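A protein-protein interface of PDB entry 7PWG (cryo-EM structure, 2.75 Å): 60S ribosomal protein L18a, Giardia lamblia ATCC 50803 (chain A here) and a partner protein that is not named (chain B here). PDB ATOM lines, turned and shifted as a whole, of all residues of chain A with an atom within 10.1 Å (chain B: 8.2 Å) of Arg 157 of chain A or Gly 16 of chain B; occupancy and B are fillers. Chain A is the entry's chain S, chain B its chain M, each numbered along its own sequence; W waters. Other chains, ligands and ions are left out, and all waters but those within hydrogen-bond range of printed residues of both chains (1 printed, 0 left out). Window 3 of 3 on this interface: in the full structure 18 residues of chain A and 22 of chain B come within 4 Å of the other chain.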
ATOM      1  N   HIS A 148     -13.956 -22.087  -5.036  1.00  0.00           N
ATOM      2  CA  HIS A 148     -13.672 -22.868  -3.843  1.00  0.00           C
ATOM      3  C   HIS A 148     -14.968 -23.159  -3.095  1.00  0.00           C
ATOM      4  O   HIS A 148     -15.733 -22.231  -2.808  1.00  0.00           O
ATOM      5  CB  HIS A 148     -12.691 -22.132  -2.938  1.00  0.00           C
ATOM      6  CG  HIS A 148     -11.964 -23.015  -1.972  1.00  0.00           C
ATOM      7  ND1 HIS A 148     -12.599 -23.945  -1.181  1.00  0.00           N
ATOM      8  CD2 HIS A 148     -10.652 -23.091  -1.653  1.00  0.00           C
ATOM      9  CE1 HIS A 148     -11.710 -24.562  -0.426  1.00  0.00           C
ATOM     10  NE2 HIS A 148     -10.521 -24.060  -0.690  1.00  0.00           N
ATOM     11  N   CYS A 150     -15.609 -23.946  -0.012  1.00  0.00           N
ATOM     12  CA  CYS A 150     -15.736 -23.549   1.389  1.00  0.00           C
ATOM     13  C   CYS A 150     -14.566 -22.707   1.892  1.00  0.00           C
ATOM     14  O   CYS A 150     -13.847 -23.146   2.791  1.00  0.00           O
ATOM     15  CB  CYS A 150     -15.878 -24.793   2.275  1.00  0.00           C
ATOM     16  SG  CYS A 150     -14.607 -26.069   2.058  1.00  0.00           S
ATOM     17  N   PRO A 151     -14.358 -21.488   1.386  1.00  0.00           N
ATOM     18  CA  PRO A 151     -13.162 -20.723   1.783  1.00  0.00           C
ATOM     19  C   PRO A 151     -13.237 -20.141   3.187  1.00  0.00           C
ATOM     20  O   PRO A 151     -12.215 -19.707   3.710  1.00  0.00           O
ATOM     21  CB  PRO A 151     -13.085 -19.612   0.725  1.00  0.00           C
ATOM     22  CG  PRO A 151     -14.231 -19.906  -0.246  1.00  0.00           C
ATOM     23  CD  PRO A 151     -15.211 -20.713   0.481  1.00  0.00           C
ATOM     24  N   TYR A 152     -14.413 -20.099   3.797  1.00  0.00           N
ATOM     25  CA  TYR A 152     -14.538 -19.673   5.180  1.00  0.00           C
ATOM     26  C   TYR A 152     -13.757 -20.573   6.128  1.00  0.00           C
ATOM     27  O   TYR A 152     -13.391 -20.132   7.219  1.00  0.00           O
ATOM     28  CB  TYR A 152     -16.014 -19.664   5.569  1.00  0.00           C
ATOM     29  CG  TYR A 152     -16.581 -21.048   5.712  1.00  0.00           C
ATOM     30  CD1 TYR A 152     -17.006 -21.762   4.614  1.00  0.00           C
ATOM     31  CD2 TYR A 152     -16.664 -21.651   6.948  1.00  0.00           C
ATOM     32  CE1 TYR A 152     -17.500 -23.020   4.747  1.00  0.00           C
ATOM     33  CE2 TYR A 152     -17.162 -22.906   7.088  1.00  0.00           C
ATOM     34  CZ  TYR A 152     -17.568 -23.590   5.989  1.00  0.00           C
ATOM     35  OH  TYR A 152     -18.065 -24.855   6.143  1.00  0.00           O
ATOM     36  N   VAL A 153     -13.512 -21.824   5.733  1.00  0.00           N
ATOM     37  CA  VAL A 153     -12.847 -22.798   6.593  1.00  0.00           C
ATOM     38  C   VAL A 153     -11.419 -22.368   6.876  1.00  0.00           C
ATOM     39  O   VAL A 153     -10.891 -22.597   7.968  1.00  0.00           O
ATOM     40  CB  VAL A 153     -12.909 -24.200   5.946  1.00  0.00           C
ATOM     41  CG1 VAL A 153     -11.981 -25.164   6.623  1.00  0.00           C
ATOM     42  CG2 VAL A 153     -14.316 -24.741   5.990  1.00  0.00           C
ATOM     43  N   HIS A 154     -10.771 -21.739   5.898  1.00  0.00           N
ATOM     44  CA  HIS A 154      -9.428 -21.210   6.104  1.00  0.00           C
ATOM     45  C   HIS A 154      -9.403 -20.126   7.169  1.00  0.00           C
ATOM     46  O   HIS A 154      -8.510 -20.109   8.018  1.00  0.00           O
ATOM     47  CB  HIS A 154      -8.879 -20.651   4.800  1.00  0.00           C
ATOM     48  CG  HIS A 154      -8.748 -21.666   3.715  1.00  0.00           C
ATOM     49  ND1 HIS A 154      -8.444 -22.983   3.961  1.00  0.00           N
ATOM     50  CD2 HIS A 154      -8.888 -21.556   2.376  1.00  0.00           C
ATOM     51  CE1 HIS A 154      -8.397 -23.641   2.820  1.00  0.00           C
ATOM     52  NE2 HIS A 154      -8.661 -22.797   1.843  1.00  0.00           N
ATOM     53  N   VAL A 155     -10.364 -19.201   7.126  1.00  0.00           N
ATOM     54  CA  VAL A 155     -10.319 -18.022   7.984  1.00  0.00           C
ATOM     55  C   VAL A 155     -10.575 -18.400   9.436  1.00  0.00           C
ATOM     56  O   VAL A 155      -9.900 -17.901  10.345  1.00  0.00           O
ATOM     57  CB  VAL A 155     -11.316 -16.958   7.488  1.00  0.00           C
ATOM     58  CG1 VAL A 155     -11.037 -15.619   8.136  1.00  0.00           C
ATOM     59  CG2 VAL A 155     -11.255 -16.825   5.995  1.00  0.00           C
ATOM     60  N   LYS A 156     -11.549 -19.280   9.675  1.00  0.00           N
ATOM     61  CA  LYS A 156     -11.873 -19.705  11.033  1.00  0.00           C
ATOM     62  C   LYS A 156     -10.693 -20.385  11.705  1.00  0.00           C
ATOM     63  O   LYS A 156     -10.455 -20.189  12.898  1.00  0.00           O
ATOM     64  CB  LYS A 156     -13.057 -20.673  11.032  1.00  0.00           C
ATOM     65  CG  LYS A 156     -14.375 -20.079  10.744  1.00  0.00           C
ATOM     66  CD  LYS A 156     -15.412 -21.163  10.629  1.00  0.00           C
ATOM     67  CE  LYS A 156     -15.467 -22.028  11.853  1.00  0.00           C
ATOM     68  NZ  LYS A 156     -16.313 -23.217  11.638  1.00  0.00           N
ATOM     69  N   ARG A 157      -9.986 -21.231  10.966  1.00  0.00           N
ATOM     70  CA  ARG A 157      -8.880 -21.984  11.538  1.00  0.00           C
ATOM     71  C   ARG A 157      -7.808 -21.056  12.083  1.00  0.00           C
ATOM     72  O   ARG A 157      -7.309 -21.259  13.195  1.00  0.00           O
ATOM     73  CB  ARG A 157      -8.306 -22.918  10.478  1.00  0.00           C
ATOM     74  CG  ARG A 157      -7.309 -23.920  10.992  1.00  0.00           C
ATOM     75  CD  ARG A 157      -6.287 -24.290   9.933  1.00  0.00           C
ATOM     76  NE  ARG A 157      -6.875 -24.679   8.657  1.00  0.00           N
ATOM     77  CZ  ARG A 157      -6.663 -24.045   7.510  1.00  0.00           C
ATOM     78  NH1 ARG A 157      -5.877 -22.980   7.472  1.00  0.00           N
ATOM     79  NH2 ARG A 157      -7.234 -24.472   6.399  1.00  0.00           N
ATOM     80  N   ALA A 158      -7.457 -20.015  11.326  1.00  0.00           N
ATOM     81  CA  ALA A 158      -6.480 -19.050  11.804  1.00  0.00           C
ATOM     82  C   ALA A 158      -6.964 -18.329  13.055  1.00  0.00           C
ATOM     83  O   ALA A 158      -6.149 -17.898  13.872  1.00  0.00           O
ATOM     84  CB  ALA A 158      -6.152 -18.050  10.699  1.00  0.00           C
ATOM     85  N   ALA A 159      -8.272 -18.201  13.228  1.00  0.00           N
ATOM     86  CA  ALA A 159      -8.864 -17.547  14.381  1.00  0.00           C
ATOM     87  C   ALA A 159      -8.954 -18.448  15.596  1.00  0.00           C
ATOM     88  O   ALA A 159      -9.727 -18.149  16.507  1.00  0.00           O
ATOM     89  CB  ALA A 159     -10.255 -17.015  14.033  1.00  0.00           C
ATOM     90  N   ARG A 160      -8.204 -19.542  15.649  1.00  0.00           N
ATOM     91  CA  ARG A 160      -8.203 -20.368  16.845  1.00  0.00           C
ATOM     92  C   ARG A 160      -7.026 -20.075  17.754  1.00  0.00           C
ATOM     93  O   ARG A 160      -7.117 -20.322  18.958  1.00  0.00           O
ATOM     94  CB  ARG A 160      -8.207 -21.854  16.484  1.00  0.00           C
ATOM     95  CG  ARG A 160      -8.577 -22.744  17.656  1.00  0.00           C
ATOM     96  CD  ARG A 160      -7.963 -24.119  17.568  1.00  0.00           C
ATOM     97  NE  ARG A 160      -8.390 -24.814  16.363  1.00  0.00           N
ATOM     98  CZ  ARG A 160      -9.615 -25.289  16.183  1.00  0.00           C
ATOM     99  NH1 ARG A 160     -10.527 -25.131  17.127  1.00  0.00           N
ATOM    100  NH2 ARG A 160      -9.933 -25.906  15.058  1.00  0.00           N
ATOM    101  N   THR A 161      -5.913 -19.578  17.214  1.00  0.00           N
ATOM    102  CA  THR A 161      -4.857 -18.998  18.036  1.00  0.00           C
ATOM    103  C   THR A 161      -4.943 -17.484  18.085  1.00  0.00           C
ATOM    104  O   THR A 161      -4.790 -16.893  19.155  1.00  0.00           O
ATOM    105  CB  THR A 161      -3.470 -19.414  17.531  1.00  0.00           C
ATOM    106  OG1 THR A 161      -3.129 -18.654  16.369  1.00  0.00           O
ATOM    107  CG2 THR A 161      -3.449 -20.884  17.179  1.00  0.00           C
ATOM    108  N   ALA A 162      -5.226 -16.844  16.953  1.00  0.00           N
ATOM    109  CA  ALA A 162      -5.452 -15.402  16.893  1.00  0.00           C
ATOM    110  C   ALA A 162      -6.870 -15.099  17.378  1.00  0.00           C
ATOM    111  O   ALA A 162      -7.763 -14.722  16.620  1.00  0.00           O
ATOM    112  CB  ALA A 162      -5.226 -14.889  15.481  1.00  0.00           C
ATOM    113  N   ARG A 163      -7.052 -15.243  18.688  1.00  0.00           N
ATOM    114  CA  ARG A 163      -8.381 -15.180  19.275  1.00  0.00           C
ATOM    115  C   ARG A 163      -8.985 -13.779  19.205  1.00  0.00           C
ATOM    116  O   ARG A 163     -10.201 -13.643  19.045  1.00  0.00           O
ATOM    117  CB  ARG A 163      -8.320 -15.676  20.713  1.00  0.00           C
ATOM    118  CG  ARG A 163      -9.573 -15.434  21.494  1.00  0.00           C
ATOM    119  CD  ARG A 163      -9.476 -16.008  22.869  1.00  0.00           C
ATOM    120  NE  ARG A 163      -9.549 -17.457  22.854  1.00  0.00           N
ATOM    121  CZ  ARG A 163     -10.131 -18.167  23.806  1.00  0.00           C
ATOM    122  NH1 ARG A 163     -10.690 -17.557  24.838  1.00  0.00           N
ATOM    123  NH2 ARG A 163     -10.157 -19.485  23.719  1.00  0.00           N
ATOM    124  N   GLN A 165      -8.627  -9.849  17.339  1.00  0.00           N
ATOM    125  CA  GLN A 165      -8.094  -9.163  16.171  1.00  0.00           C
ATOM    126  C   GLN A 165      -8.614  -7.734  16.177  1.00  0.00           C
ATOM    127  O   GLN A 165      -9.448  -7.374  17.002  1.00  0.00           O
ATOM    128  CB  GLN A 165      -8.481  -9.908  14.896  1.00  0.00           C
ATOM    129  CG  GLN A 165      -8.016 -11.343  14.908  1.00  0.00           C
ATOM    130  CD  GLN A 165      -8.105 -12.001  13.569  1.00  0.00           C
ATOM    131  OE1 GLN A 165      -8.028 -11.343  12.544  1.00  0.00           O
ATOM    132  NE2 GLN A 165      -8.280 -13.311  13.566  1.00  0.00           N
ATOM    133  N   PRO A 169     -11.879 -10.226   9.518  1.00  0.00           N
ATOM    134  CA  PRO A 169     -11.225 -10.580   8.257  1.00  0.00           C
ATOM    135  C   PRO A 169     -12.205 -10.908   7.144  1.00  0.00           C
ATOM    136  O   PRO A 169     -13.353 -11.298   7.366  1.00  0.00           O
ATOM    137  CB  PRO A 169     -10.393 -11.810   8.631  1.00  0.00           C
ATOM    138  CG  PRO A 169     -11.022 -12.335   9.851  1.00  0.00           C
ATOM    139  CD  PRO A 169     -11.498 -11.149  10.596  1.00  0.00           C
ATOM    140  N   VAL A 171     -13.020 -12.929   3.311  1.00  0.00           N
ATOM    141  CA  VAL A 171     -12.894 -14.278   2.764  1.00  0.00           C
ATOM    142  C   VAL A 171     -12.603 -14.154   1.273  1.00  0.00           C
ATOM    143  O   VAL A 171     -13.534 -14.014   0.473  1.00  0.00           O
ATOM    144  CB  VAL A 171     -14.152 -15.114   3.043  1.00  0.00           C
ATOM    145  CG1 VAL A 171     -13.833 -16.566   3.012  1.00  0.00           C
ATOM    146  CG2 VAL A 171     -14.753 -14.759   4.394  1.00  0.00           C
ATOM    147  N   VAL B  13      -1.548 -23.378  -5.230  1.00  0.00           N
ATOM    148  CA  VAL B  13      -2.167 -23.284  -3.915  1.00  0.00           C
ATOM    149  C   VAL B  13      -1.090 -23.257  -2.841  1.00  0.00           C
ATOM    150  O   VAL B  13       0.034 -23.711  -3.040  1.00  0.00           O
ATOM    151  CB  VAL B  13      -3.153 -24.438  -3.624  1.00  0.00           C
ATOM    152  CG1 VAL B  13      -4.157 -24.617  -4.765  1.00  0.00           C
ATOM    153  CG2 VAL B  13      -2.405 -25.725  -3.341  1.00  0.00           C
ATOM    154  N   TYR B  14      -1.461 -22.717  -1.689  1.00  0.00           N
ATOM    155  CA  TYR B  14      -0.622 -22.675  -0.505  1.00  0.00           C
ATOM    156  C   TYR B  14      -1.247 -23.573   0.552  1.00  0.00           C
ATOM    157  O   TYR B  14      -2.445 -23.466   0.827  1.00  0.00           O
ATOM    158  CB  TYR B  14      -0.482 -21.236  -0.008  1.00  0.00           C
ATOM    159  CG  TYR B  14       0.337 -21.056   1.236  1.00  0.00           C
ATOM    160  CD1 TYR B  14       1.698 -21.252   1.216  1.00  0.00           C
ATOM    161  CD2 TYR B  14      -0.252 -20.666   2.424  1.00  0.00           C
ATOM    162  CE1 TYR B  14       2.443 -21.092   2.335  1.00  0.00           C
ATOM    163  CE2 TYR B  14       0.492 -20.498   3.552  1.00  0.00           C
ATOM    164  CZ  TYR B  14       1.845 -20.714   3.500  1.00  0.00           C
ATOM    165  OH  TYR B  14       2.618 -20.547   4.622  1.00  0.00           O
ATOM    166  N   LEU B  15      -0.455 -24.480   1.116  1.00  0.00           N
ATOM    167  CA  LEU B  15      -1.001 -25.489   2.017  1.00  0.00           C
ATOM    168  C   LEU B  15      -1.126 -24.924   3.424  1.00  0.00           C
ATOM    169  O   LEU B  15      -0.129 -24.538   4.041  1.00  0.00           O
ATOM    170  CB  LEU B  15      -0.139 -26.743   1.998  1.00  0.00           C
ATOM    171  CG  LEU B  15      -0.218 -27.458   0.652  1.00  0.00           C
ATOM    172  CD1 LEU B  15       0.724 -28.639   0.618  1.00  0.00           C
ATOM    173  CD2 LEU B  15      -1.642 -27.902   0.362  1.00  0.00           C
ATOM    174  N   GLY B  16      -2.356 -24.874   3.925  1.00  0.00           N
ATOM    175  CA  GLY B  16      -2.662 -24.290   5.208  1.00  0.00           C
ATOM    176  C   GLY B  16      -2.838 -25.260   6.348  1.00  0.00           C
ATOM    177  O   GLY B  16      -3.005 -24.826   7.488  1.00  0.00           O
ATOM    178  N   ASP B  17      -2.802 -26.558   6.088  1.00  0.00           N
ATOM    179  CA  ASP B  17      -2.952 -27.534   7.154  1.00  0.00           C
ATOM    180  C   ASP B  17      -2.406 -28.865   6.668  1.00  0.00           C
ATOM    181  O   ASP B  17      -2.121 -29.045   5.487  1.00  0.00           O
ATOM    182  CB  ASP B  17      -4.409 -27.664   7.602  1.00  0.00           C
ATOM    183  CG  ASP B  17      -4.531 -28.113   9.031  1.00  0.00           C
ATOM    184  OD1 ASP B  17      -3.589 -28.751   9.525  1.00  0.00           O
ATOM    185  OD2 ASP B  17      -5.559 -27.834   9.664  1.00  0.00           O
ATOM    186  N   GLY B  18      -2.278 -29.798   7.600  1.00  0.00           N
ATOM    187  CA  GLY B  18      -1.709 -31.088   7.315  1.00  0.00           C
ATOM    188  C   GLY B  18      -0.258 -31.150   7.734  1.00  0.00           C
ATOM    189  O   GLY B  18       0.234 -30.290   8.468  1.00  0.00           O
ATOM    190  N   PRO B  19       0.457 -32.186   7.290  1.00  0.00           N
ATOM    191  CA  PRO B  19       1.893 -32.268   7.576  1.00  0.00           C
ATOM    192  C   PRO B  19       2.764 -31.500   6.596  1.00  0.00           C
ATOM    193  O   PRO B  19       3.945 -31.275   6.889  1.00  0.00           O
ATOM    194  CB  PRO B  19       2.169 -33.769   7.504  1.00  0.00           C
ATOM    195  CG  PRO B  19       1.167 -34.285   6.566  1.00  0.00           C
ATOM    196  CD  PRO B  19      -0.051 -33.413   6.658  1.00  0.00           C
ATOM    197  N   ASP B  20       2.227 -31.089   5.449  1.00  0.00           N
ATOM    198  CA  ASP B  20       2.935 -30.236   4.508  1.00  0.00           C
ATOM    199  C   ASP B  20       2.546 -28.777   4.651  1.00  0.00           C
ATOM    200  O   ASP B  20       2.790 -27.989   3.736  1.00  0.00           O
ATOM    201  CB  ASP B  20       2.690 -30.707   3.077  1.00  0.00           C
ATOM    202  CG  ASP B  20       3.734 -31.695   2.613  1.00  0.00           C
ATOM    203  OD1 ASP B  20       4.848 -31.661   3.163  1.00  0.00           O
ATOM    204  OD2 ASP B  20       3.452 -32.499   1.706  1.00  0.00           O
ATOM    205  N   LYS B  21       1.947 -28.406   5.776  1.00  0.00           N
ATOM    206  CA  LYS B  21       1.564 -27.022   6.018  1.00  0.00           C
ATOM    207  C   LYS B  21       2.746 -26.082   5.808  1.00  0.00           C
ATOM    208  O   LYS B  21       3.878 -26.392   6.176  1.00  0.00           O
ATOM    209  CB  LYS B  21       1.022 -26.891   7.440  1.00  0.00           C
ATOM    210  CG  LYS B  21       1.153 -25.534   8.047  1.00  0.00           C
ATOM    211  CD  LYS B  21       0.596 -25.538   9.450  1.00  0.00           C
ATOM    212  CE  LYS B  21       0.775 -24.196  10.111  1.00  0.00           C
ATOM    213  NZ  LYS B  21       0.417 -24.265  11.542  1.00  0.00           N
ATOM    214  N   GLY B  22       2.473 -24.942   5.170  1.00  0.00           N
ATOM    215  CA  GLY B  22       3.460 -23.909   4.935  1.00  0.00           C
ATOM    216  C   GLY B  22       4.093 -23.888   3.560  1.00  0.00           C
ATOM    217  O   GLY B  22       4.905 -22.997   3.294  1.00  0.00           O
ATOM    218  N   LYS B  23       3.725 -24.805   2.670  1.00  0.00           N
ATOM    219  CA  LYS B  23       4.397 -24.995   1.393  1.00  0.00           C
ATOM    220  C   LYS B  23       3.460 -24.699   0.229  1.00  0.00           C
ATOM    221  O   LYS B  23       2.241 -24.669   0.374  1.00  0.00           O
ATOM    222  CB  LYS B  23       4.922 -26.426   1.266  1.00  0.00           C
ATOM    223  CG  LYS B  23       5.925 -26.832   2.331  1.00  0.00           C
ATOM    224  CD  LYS B  23       6.046 -28.351   2.419  1.00  0.00           C
ATOM    225  CE  LYS B  23       7.394 -28.773   2.963  1.00  0.00           C
ATOM    226  NZ  LYS B  23       7.715 -28.118   4.258  1.00  0.00           N
ATOM    227  N   LEU B  24       4.052 -24.493  -0.939  1.00  0.00           N
ATOM    228  CA  LEU B  24       3.323 -24.311  -2.183  1.00  0.00           C
ATOM    229  C   LEU B  24       3.284 -25.617  -2.964  1.00  0.00           C
ATOM    230  O   LEU B  24       4.067 -26.533  -2.718  1.00  0.00           O
ATOM    231  CB  LEU B  24       3.962 -23.210  -3.026  1.00  0.00           C
ATOM    232  CG  LEU B  24       3.734 -21.793  -2.512  1.00  0.00           C
ATOM    233  CD1 LEU B  24       4.816 -20.863  -3.013  1.00  0.00           C
ATOM    234  CD2 LEU B  24       2.371 -21.307  -2.951  1.00  0.00           C
ATOM    235  N   SER B  51      -7.361 -32.662   1.071  1.00  0.00           N
ATOM    236  CA  SER B  51      -8.707 -32.129   1.182  1.00  0.00           C
ATOM    237  C   SER B  51      -8.701 -30.647   0.828  1.00  0.00           C
ATOM    238  O   SER B  51      -7.813 -29.903   1.244  1.00  0.00           O
ATOM    239  CB  SER B  51      -9.222 -32.338   2.602  1.00  0.00           C
ATOM    240  OG  SER B  51     -10.371 -31.578   2.866  1.00  0.00           O
ATOM    241  N   LEU B  52      -9.710 -30.215   0.069  1.00  0.00           N
ATOM    242  CA  LEU B  52      -9.772 -28.816  -0.334  1.00  0.00           C
ATOM    243  C   LEU B  52      -9.874 -27.869   0.855  1.00  0.00           C
ATOM    244  O   LEU B  52      -9.542 -26.689   0.721  1.00  0.00           O
ATOM    245  CB  LEU B  52     -10.931 -28.604  -1.308  1.00  0.00           C
ATOM    246  CG  LEU B  52     -10.505 -28.768  -2.775  1.00  0.00           C
ATOM    247  CD1 LEU B  52     -11.684 -28.932  -3.681  1.00  0.00           C
ATOM    248  CD2 LEU B  52      -9.675 -27.592  -3.223  1.00  0.00           C
ATOM    249  N   ARG B  53     -10.281 -28.369   2.022  1.00  0.00           N
ATOM    250  CA  ARG B  53     -10.228 -27.592   3.251  1.00  0.00           C
ATOM    251  C   ARG B  53      -8.808 -27.199   3.645  1.00  0.00           C
ATOM    252  O   ARG B  53      -8.644 -26.308   4.481  1.00  0.00           O
ATOM    253  CB  ARG B  53     -10.874 -28.380   4.385  1.00  0.00           C
ATOM    254  CG  ARG B  53     -12.374 -28.560   4.280  1.00  0.00           C
ATOM    255  CD  ARG B  53     -12.881 -29.619   5.231  1.00  0.00           C
ATOM    256  NE  ARG B  53     -12.640 -29.301   6.632  1.00  0.00           N
ATOM    257  CZ  ARG B  53     -13.510 -28.677   7.417  1.00  0.00           C
ATOM    258  NH1 ARG B  53     -14.680 -28.299   6.942  1.00  0.00           N
ATOM    259  NH2 ARG B  53     -13.211 -28.429   8.673  1.00  0.00           N
ATOM    260  N   TRP B  54      -7.775 -27.834   3.088  1.00  0.00           N
ATOM    261  CA  TRP B  54      -6.397 -27.478   3.424  1.00  0.00           C
ATOM    262  C   TRP B  54      -5.750 -26.518   2.439  1.00  0.00           C
ATOM    263  O   TRP B  54      -4.737 -25.902   2.778  1.00  0.00           O
ATOM    264  CB  TRP B  54      -5.504 -28.720   3.505  1.00  0.00           C
ATOM    265  CG  TRP B  54      -5.702 -29.595   4.677  1.00  0.00           C
ATOM    266  CD1 TRP B  54      -6.485 -29.361   5.749  1.00  0.00           C
ATOM    267  CD2 TRP B  54      -5.104 -30.873   4.890  1.00  0.00           C
ATOM    268  NE1 TRP B  54      -6.413 -30.403   6.629  1.00  0.00           N
ATOM    269  CE2 TRP B  54      -5.568 -31.349   6.121  1.00  0.00           C
ATOM    270  CE3 TRP B  54      -4.222 -31.662   4.155  1.00  0.00           C
ATOM    271  CZ2 TRP B  54      -5.182 -32.577   6.637  1.00  0.00           C
ATOM    272  CZ3 TRP B  54      -3.845 -32.873   4.663  1.00  0.00           C
ATOM    273  CH2 TRP B  54      -4.323 -33.323   5.892  1.00  0.00           C
ATOM    274  N   ALA B  55      -6.294 -26.386   1.237  1.00  0.00           N
ATOM    275  CA  ALA B  55      -5.650 -25.670   0.150  1.00  0.00           C
ATOM    276  C   ALA B  55      -6.200 -24.259   0.052  1.00  0.00           C
ATOM    277  O   ALA B  55      -7.416 -24.072  -0.023  1.00  0.00           O
ATOM    278  CB  ALA B  55      -5.868 -26.407  -1.164  1.00  0.00           C
ATOM    279  N   MET B  56      -5.316 -23.268   0.060  1.00  0.00           N
ATOM    280  CA  MET B  56      -5.709 -21.878  -0.128  1.00  0.00           C
ATOM    281  C   MET B  56      -5.379 -21.472  -1.556  1.00  0.00           C
ATOM    282  O   MET B  56      -4.230 -21.575  -1.980  1.00  0.00           O
ATOM    283  CB  MET B  56      -5.014 -20.949   0.867  1.00  0.00           C
ATOM    284  CG  MET B  56      -5.191 -21.308   2.317  1.00  0.00           C
ATOM    285  SD  MET B  56      -4.839 -19.918   3.391  1.00  0.00           S
ATOM    286  CE  MET B  56      -4.072 -20.749   4.766  1.00  0.00           C
HETATM  287  O   HOH W   1     -16.412 -28.110   4.130  1.00  0.00           O
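The guanidinium group (NH1) of Arg 157 of chain A sits at hydrogen-bond distance from the backbone carbonyl oxygen (O) of Gly 16 of chain B (3.4 Å).
OD2 of Asp 17 of chain B lies within salt-bridge range of NE of Arg 157 of chain A, 3.6 Å away.
The backbone carbonyl oxygen (O) of Leu 52 of chain B is in hydrogen-bond range of a ring nitrogen (NE2) of His 148 of chain A (3.1 Å).
ND1 of His 154 of chain A lies close to O of Arg 53 of chain B (3.4 Å).
The guanidinium group (NH2) of Arg 157 of chain A is in hydrogen-bond range of the backbone carbonyl oxygen (O) of Arg 53 of chain B.
The backbone carbonyl oxygen of Ala 55 of chain B lies within hydrogen-bond range of a ring nitrogen (NE2) of His 148 of chain A (3.2 Å).
The backbone carbonyl oxygen (O) of Ala 55 of chain B sits at hydrogen-bond distance from a ring nitrogen (NE2) of His 154 of chain A, 2.6 Å away.
O of Tyr 14 of chain B lies within hydrogen-bond range of N of Met 56 of chain B, at 3.0 Å.
O of Trp 54 of chain B is in hydrogen-bond range of N of Gly 16 of chain B, at 2.8 Å.
N of Arg 53 of chain B sits close to OG of Ser 51 of chain B (3.3 Å).
A ring nitrogen (ND1) of His 148 of chain A sits at hydrogen-bond distance from the backbone NH of Cys 150 of chain A, 3.2 Å away.
A ring nitrogen (NE2) of His 148 of chain A is in hydrogen-bond range of a ring nitrogen (NE2) of His 154 of chain A, at 3.4 Å.
ND1 of His 154 of chain A lies within hydrogen-bond range of NH2 of Arg 157 of chain A (3.1 Å).
Val 153 of chain A touches Arg 53 of chain B (CG2 to NH1, 3.7 Å).
Leu 52 of chain B touches His 154 of chain A (O to CE1, 3.9 Å).
Trp 54 of chain B touches His 154 of chain A.
NE2 of His 154 of chain A touches CA of Met 56 of chain B, 3.7 Å away.
NH1 of Arg 157 of chain A touches CE of Met 56 of chain B, 3.9 Å away.
Of the printed residues of chain B, His 154 of chain A touches Leu 52, Arg 53, Trp 54, Ala 55 and Met 56.
Arg 157 of chain A touches just these residues of chain B: Gly 16 (3.4 Å), Asp 17 (3.6 Å), Arg 53 (3.0 Å) and Met 56 (3.9 Å).
No residue of chain B comes within 4 Å of Ala 158 of chain A.
No residue of chain A comes within 4 Å of Leu 15 of chain B.
Gly 16 of chain B touches just one residue of chain A: Arg 157.
Of chain A, only Arg 157 (3.6 Å) comes within 4 Å of Asp 17 of chain B.
Gly 18 of chain B touches none of the printed residues of chain A.
Lys 21 of chain B touches none of the printed residues of chain A.
Of the printed residues of chain A, Leu 52 of chain B touches His 148 and His 154.
Of the 18 printed residues of chain B, 7 touch a printed residue of chain A.
Hydrophobic or aromatic side chains of chain B that line the printed part of chain A: Met 56.
Among the printed residues, Asp or Glu carboxylates within 4 Å of a Lys or Arg side-chain nitrogen of the other chain: Arg 157 of chain A with Asp 17 of chain B (3.6 Å).
Water W1 lies within hydrogen-bond range of the guanidinium group (NH1) of Arg 53 of chain B (3.3 Å) and the side-chain sulfur (SG) of Cys 150 of chain A (3.4 Å).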
